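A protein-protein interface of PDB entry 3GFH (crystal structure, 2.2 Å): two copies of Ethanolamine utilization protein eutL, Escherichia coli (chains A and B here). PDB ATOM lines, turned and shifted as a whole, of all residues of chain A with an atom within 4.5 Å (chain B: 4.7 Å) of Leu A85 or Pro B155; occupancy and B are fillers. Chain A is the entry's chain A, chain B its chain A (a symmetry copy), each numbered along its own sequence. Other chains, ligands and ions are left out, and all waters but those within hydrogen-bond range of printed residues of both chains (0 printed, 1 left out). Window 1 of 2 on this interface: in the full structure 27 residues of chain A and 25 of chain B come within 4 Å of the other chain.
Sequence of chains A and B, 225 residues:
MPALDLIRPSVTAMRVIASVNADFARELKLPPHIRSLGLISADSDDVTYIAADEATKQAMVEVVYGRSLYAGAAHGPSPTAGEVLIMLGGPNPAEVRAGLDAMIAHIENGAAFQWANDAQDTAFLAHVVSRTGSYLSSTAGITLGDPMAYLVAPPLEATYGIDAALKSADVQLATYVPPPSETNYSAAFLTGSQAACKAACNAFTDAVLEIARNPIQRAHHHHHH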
ATOM      1  N   ILE A  40       9.999 -10.063  26.241  1.00  0.00           N
ATOM      2  CA  ILE A  40      11.224  -9.840  25.503  1.00  0.00           C
ATOM      3  C   ILE A  40      11.519 -11.103  24.711  1.00  0.00           C
ATOM      4  O   ILE A  40      11.397 -12.194  25.233  1.00  0.00           O
ATOM      5  CB  ILE A  40      12.369  -9.395  26.471  1.00  0.00           C
ATOM      6  CG1 ILE A  40      13.597  -8.937  25.707  1.00  0.00           C
ATOM      7  CG2 ILE A  40      12.744 -10.486  27.508  1.00  0.00           C
ATOM      8  CD1 ILE A  40      14.779  -8.633  26.650  1.00  0.00           C
ATOM      9  N   TYR A  65       7.857 -16.539  33.243  1.00  0.00           N
ATOM     10  CA  TYR A  65       7.771 -17.540  32.244  1.00  0.00           C
ATOM     11  C   TYR A  65       9.035 -17.472  31.453  1.00  0.00           C
ATOM     12  O   TYR A  65       9.815 -16.518  31.596  1.00  0.00           O
ATOM     13  CB  TYR A  65       6.502 -17.322  31.392  1.00  0.00           C
ATOM     14  CG  TYR A  65       6.288 -18.312  30.276  1.00  0.00           C
ATOM     15  CD1 TYR A  65       5.522 -19.463  30.463  1.00  0.00           C
ATOM     16  CD2 TYR A  65       6.812 -18.069  28.996  1.00  0.00           C
ATOM     17  CE1 TYR A  65       5.311 -20.365  29.417  1.00  0.00           C
ATOM     18  CE2 TYR A  65       6.628 -18.960  27.982  1.00  0.00           C
ATOM     19  CZ  TYR A  65       5.871 -20.097  28.178  1.00  0.00           C
ATOM     20  OH  TYR A  65       5.678 -20.961  27.108  1.00  0.00           O
ATOM     21  N   GLY A  66       9.275 -18.515  30.662  1.00  0.00           N
ATOM     22  CA  GLY A  66      10.337 -18.457  29.656  1.00  0.00           C
ATOM     23  C   GLY A  66      10.665 -19.858  29.190  1.00  0.00           C
ATOM     24  O   GLY A  66      10.801 -20.750  30.013  1.00  0.00           O
ATOM     25  N   ARG A  67      10.750 -19.995  27.873  1.00  0.00           N
ATOM     26  CA  ARG A  67      10.835 -21.254  27.124  1.00  0.00           C
ATOM     27  C   ARG A  67      11.329 -20.871  25.694  1.00  0.00           C
ATOM     28  O   ARG A  67      11.255 -19.683  25.308  1.00  0.00           O
ATOM     29  CB  ARG A  67       9.482 -21.949  27.047  1.00  0.00           C
ATOM     30  CG  ARG A  67       9.135 -22.742  28.363  1.00  0.00           C
ATOM     31  CD  ARG A  67       8.039 -23.800  28.129  1.00  0.00           C
ATOM     32  NE  ARG A  67       8.469 -25.085  28.689  1.00  0.00           N
ATOM     33  CZ  ARG A  67       8.612 -26.207  27.987  1.00  0.00           C
ATOM     34  NH1 ARG A  67       8.314 -26.231  26.687  1.00  0.00           N
ATOM     35  NH2 ARG A  67       9.046 -27.311  28.597  1.00  0.00           N
ATOM     36  N   LEU A  69      12.163 -22.181  21.275  1.00  0.00           N
ATOM     37  CA  LEU A  69      11.430 -22.522  20.060  1.00  0.00           C
ATOM     38  C   LEU A  69      12.036 -23.749  19.330  1.00  0.00           C
ATOM     39  O   LEU A  69      13.247 -23.883  19.201  1.00  0.00           O
ATOM     40  CB  LEU A  69      11.329 -21.302  19.123  1.00  0.00           C
ATOM     41  CG  LEU A  69      10.673 -20.007  19.669  1.00  0.00           C
ATOM     42  CD1 LEU A  69      10.670 -18.897  18.618  1.00  0.00           C
ATOM     43  CD2 LEU A  69       9.257 -20.226  20.176  1.00  0.00           C
ATOM     44  N   ALA A  81       9.961 -13.714  16.756  1.00  0.00           N
ATOM     45  CA  ALA A  81      10.066 -14.469  17.997  1.00  0.00           C
ATOM     46  C   ALA A  81      11.451 -14.979  18.349  1.00  0.00           C
ATOM     47  O   ALA A  81      11.639 -15.539  19.424  1.00  0.00           O
ATOM     48  CB  ALA A  81       9.060 -15.586  18.033  1.00  0.00           C
ATOM     49  N   VAL A  84      13.459 -17.458  21.787  1.00  0.00           N
ATOM     50  CA  VAL A  84      13.100 -17.486  23.211  1.00  0.00           C
ATOM     51  C   VAL A  84      11.964 -16.502  23.476  1.00  0.00           C
ATOM     52  O   VAL A  84      11.745 -15.619  22.676  1.00  0.00           O
ATOM     53  CB  VAL A  84      14.248 -17.027  24.164  1.00  0.00           C
ATOM     54  CG1 VAL A  84      14.300 -17.930  25.462  1.00  0.00           C
ATOM     55  CG2 VAL A  84      15.549 -17.029  23.476  1.00  0.00           C
ATOM     56  N   LEU A  85      11.281 -16.670  24.615  1.00  0.00           N
ATOM     57  CA  LEU A  85      10.363 -15.666  25.162  1.00  0.00           C
ATOM     58  C   LEU A  85      10.532 -15.691  26.677  1.00  0.00           C
ATOM     59  O   LEU A  85      10.342 -16.742  27.339  1.00  0.00           O
ATOM     60  CB  LEU A  85       8.901 -15.933  24.771  1.00  0.00           C
ATOM     61  CG  LEU A  85       7.820 -14.848  24.953  1.00  0.00           C
ATOM     62  CD1 LEU A  85       6.431 -15.417  25.003  1.00  0.00           C
ATOM     63  CD2 LEU A  85       7.970 -14.112  26.170  1.00  0.00           C
ATOM     64  N   ILE A  86      10.924 -14.541  27.229  1.00  0.00           N
ATOM     65  CA  ILE A  86      11.027 -14.384  28.669  1.00  0.00           C
ATOM     66  C   ILE A  86       9.922 -13.402  29.075  1.00  0.00           C
ATOM     67  O   ILE A  86       9.645 -12.437  28.343  1.00  0.00           O
ATOM     68  CB  ILE A  86      12.367 -13.796  29.064  1.00  0.00           C
ATOM     69  CG1 ILE A  86      13.400 -14.844  29.543  1.00  0.00           C
ATOM     70  CG2 ILE A  86      12.184 -12.869  30.213  1.00  0.00           C
ATOM     71  CD1 ILE A  86      13.211 -16.162  29.097  1.00  0.00           C
ATOM     72  N   MET A  87       9.300 -13.660  30.222  1.00  0.00           N
ATOM     73  CA  MET A  87       8.229 -12.853  30.759  1.00  0.00           C
ATOM     74  C   MET A  87       8.596 -12.470  32.194  1.00  0.00           C
ATOM     75  O   MET A  87       8.417 -13.275  33.115  1.00  0.00           O
ATOM     76  CB  MET A  87       6.895 -13.657  30.791  1.00  0.00           C
ATOM     77  CG  MET A  87       5.998 -13.572  29.562  1.00  0.00           C
ATOM     78  SD  MET A  87       4.388 -14.457  29.754  1.00  0.00           S
ATOM     79  CE  MET A  87       4.098 -14.367  31.518  1.00  0.00           C
ATOM     80  N   ALA B 153      -0.464 -16.209  17.118  1.00  0.00           N
ATOM     81  CA  ALA B 153       0.530 -15.228  16.728  1.00  0.00           C
ATOM     82  C   ALA B 153       1.828 -15.704  17.319  1.00  0.00           C
ATOM     83  O   ALA B 153       1.830 -16.565  18.214  1.00  0.00           O
ATOM     84  CB  ALA B 153       0.125 -13.812  17.264  1.00  0.00           C
ATOM     85  N   PRO B 154       2.961 -15.250  16.778  1.00  0.00           N
ATOM     86  CA  PRO B 154       4.264 -15.644  17.402  1.00  0.00           C
ATOM     87  C   PRO B 154       4.259 -15.310  18.914  1.00  0.00           C
ATOM     88  O   PRO B 154       3.318 -14.652  19.374  1.00  0.00           O
ATOM     89  CB  PRO B 154       5.258 -14.780  16.638  1.00  0.00           C
ATOM     90  CG  PRO B 154       4.587 -14.535  15.284  1.00  0.00           C
ATOM     91  CD  PRO B 154       3.136 -14.443  15.554  1.00  0.00           C
ATOM     92  N   PRO B 155       5.267 -15.753  19.699  1.00  0.00           N
ATOM     93  CA  PRO B 155       5.133 -15.663  21.186  1.00  0.00           C
ATOM     94  C   PRO B 155       4.887 -14.304  21.859  1.00  0.00           C
ATOM     95  O   PRO B 155       4.062 -14.186  22.793  1.00  0.00           O
ATOM     96  CB  PRO B 155       6.454 -16.271  21.678  1.00  0.00           C
ATOM     97  CG  PRO B 155       6.732 -17.367  20.578  1.00  0.00           C
ATOM     98  CD  PRO B 155       6.277 -16.766  19.290  1.00  0.00           C
ATOM     99  N   LEU B 156       5.586 -13.266  21.432  1.00  0.00           N
ATOM    100  CA  LEU B 156       5.479 -12.038  22.134  1.00  0.00           C
ATOM    101  C   LEU B 156       4.251 -11.368  21.614  1.00  0.00           C
ATOM    102  O   LEU B 156       3.383 -10.918  22.371  1.00  0.00           O
ATOM    103  CB  LEU B 156       6.736 -11.220  21.908  1.00  0.00           C
ATOM    104  CG  LEU B 156       6.838  -9.953  22.730  1.00  0.00           C
ATOM    105  CD1 LEU B 156       8.287  -9.682  23.157  1.00  0.00           C
ATOM    106  CD2 LEU B 156       6.333  -8.844  21.887  1.00  0.00           C
ATOM    107  N   GLU B 157       4.169 -11.301  20.295  1.00  0.00           N
ATOM    108  CA  GLU B 157       2.906 -10.894  19.663  1.00  0.00           C
ATOM    109  C   GLU B 157       1.675 -11.506  20.378  1.00  0.00           C
ATOM    110  O   GLU B 157       0.737 -10.814  20.716  1.00  0.00           O
ATOM    111  CB  GLU B 157       2.878 -11.352  18.217  1.00  0.00           C
ATOM    112  CG  GLU B 157       3.527 -10.346  17.229  1.00  0.00           C
ATOM    113  CD  GLU B 157       4.960 -10.631  16.962  1.00  0.00           C
ATOM    114  OE1 GLU B 157       5.496 -11.525  17.644  1.00  0.00           O
ATOM    115  OE2 GLU B 157       5.557  -9.953  16.057  1.00  0.00           O
ATOM    116  N   ALA B 158       1.660 -12.805  20.578  1.00  0.00           N
ATOM    117  CA  ALA B 158       0.438 -13.418  21.081  1.00  0.00           C
ATOM    118  C   ALA B 158       0.067 -12.974  22.479  1.00  0.00           C
ATOM    119  O   ALA B 158      -1.093 -12.673  22.703  1.00  0.00           O
ATOM    120  CB  ALA B 158       0.513 -14.926  21.018  1.00  0.00           C
ATOM    121  N   THR B 159       1.041 -12.960  23.384  1.00  0.00           N
ATOM    122  CA  THR B 159       0.876 -12.648  24.851  1.00  0.00           C
ATOM    123  C   THR B 159       0.265 -11.268  25.053  1.00  0.00           C
ATOM    124  O   THR B 159      -0.652 -11.090  25.834  1.00  0.00           O
ATOM    125  CB  THR B 159       2.260 -12.683  25.607  1.00  0.00           C
ATOM    126  OG1 THR B 159       2.775 -14.005  25.637  1.00  0.00           O
ATOM    127  CG2 THR B 159       2.169 -12.183  27.064  1.00  0.00           C
ATOM    128  N   PRO B 179       3.238 -19.971  24.686  1.00  0.00           N
ATOM    129  CA  PRO B 179       4.088 -19.680  23.545  1.00  0.00           C
ATOM    130  C   PRO B 179       4.477 -20.836  22.658  1.00  0.00           C
ATOM    131  O   PRO B 179       4.013 -20.871  21.507  1.00  0.00           O
ATOM    132  CB  PRO B 179       5.289 -19.051  24.202  1.00  0.00           C
ATOM    133  CG  PRO B 179       4.654 -18.231  25.354  1.00  0.00           C
ATOM    134  CD  PRO B 179       3.296 -18.857  25.644  1.00  0.00           C
ATOM    135  N   ASN B 184       5.490 -23.481  16.911  1.00  0.00           N
ATOM    136  CA  ASN B 184       6.232 -22.370  17.439  1.00  0.00           C
ATOM    137  C   ASN B 184       5.426 -21.081  17.563  1.00  0.00           C
ATOM    138  O   ASN B 184       6.011 -19.998  17.852  1.00  0.00           O
ATOM    139  CB  ASN B 184       7.556 -22.178  16.680  1.00  0.00           C
ATOM    140  CG  ASN B 184       8.578 -23.276  17.029  1.00  0.00           C
ATOM    141  OD1 ASN B 184       8.684 -23.678  18.218  1.00  0.00           O
ATOM    142  ND2 ASN B 184       9.321 -23.789  16.000  1.00  0.00           N
ATOM    143  N   SER B 186       1.759 -19.298  19.530  1.00  0.00           N
ATOM    144  CA  SER B 186       1.000 -19.320  20.767  1.00  0.00           C
ATOM    145  C   SER B 186      -0.416 -19.121  20.258  1.00  0.00           C
ATOM    146  O   SER B 186      -0.592 -18.631  19.122  1.00  0.00           O
ATOM    147  CB  SER B 186       1.402 -18.161  21.666  1.00  0.00           C
ATOM    148  OG  SER B 186       0.725 -18.182  22.919  1.00  0.00           O
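Among the printed residues, merely in contact across the chains: Ile A40 with Leu B156 (3.5 Å), Tyr A65 with Pro B179 (3.4 Å), Leu A69 with Pro B155 (3.8 Å), Leu A69 with Asn B184 (3.5 Å), Ala A81 with Pro B155 (3.3 Å), Leu A85 with Pro B155 (3.4 Å), Leu A85 with Thr B159 (3.97 Å) and Leu A85 with Pro B179 (3.3 Å).
No position is printed for both chains. Of the 8 pairs that touch across the chains among the printed residues, none has its exchanged pair printed and touching as well.
Among the printed residues, 8 pairs touch across the chains. Among the printed residues, no Asp or Glu carboxylate lies within 4 Å of a Lys or Arg side-chain nitrogen of the other chain.
The backbone carbonyl oxygen (O) of Pro B155 sits at hydrogen-bond distance from the side-chain hydroxyl (OG1) of Thr B159, 3.1 Å away. The backbone NH (N) of Ser B186 lies within hydrogen-bond range of the backbone carbonyl oxygen (O) of Pro B179, at 3.4 Å. The backbone carbonyl oxygen of Tyr A65 sits at hydrogen-bond distance from the backbone NH of Met A87. The backbone carbonyl oxygen (O) of Ile A40 lies within hydrogen-bond range of the backbone NH (N) of Ile A86 (3.1 Å). N of Leu A85 sits at hydrogen-bond distance from O of Arg A67 (3.1 Å).
Of the printed residues of chain B, Ile A40 touches Leu B156. Of the printed residues of chain B, Leu A85 touches Pro B155 (3.4 Å), Thr B159 (3.97 Å) and Pro B179 (3.3 Å). Printed residues of chain A within 4 Å of Leu B156: Ile A40. The nearest residue of chain B that does not touch Leu A85 is Leu B156 (4.3 Å). The nearest printed residue of chain B that does not touch Tyr A65 is Thr B159 (6.6 Å).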
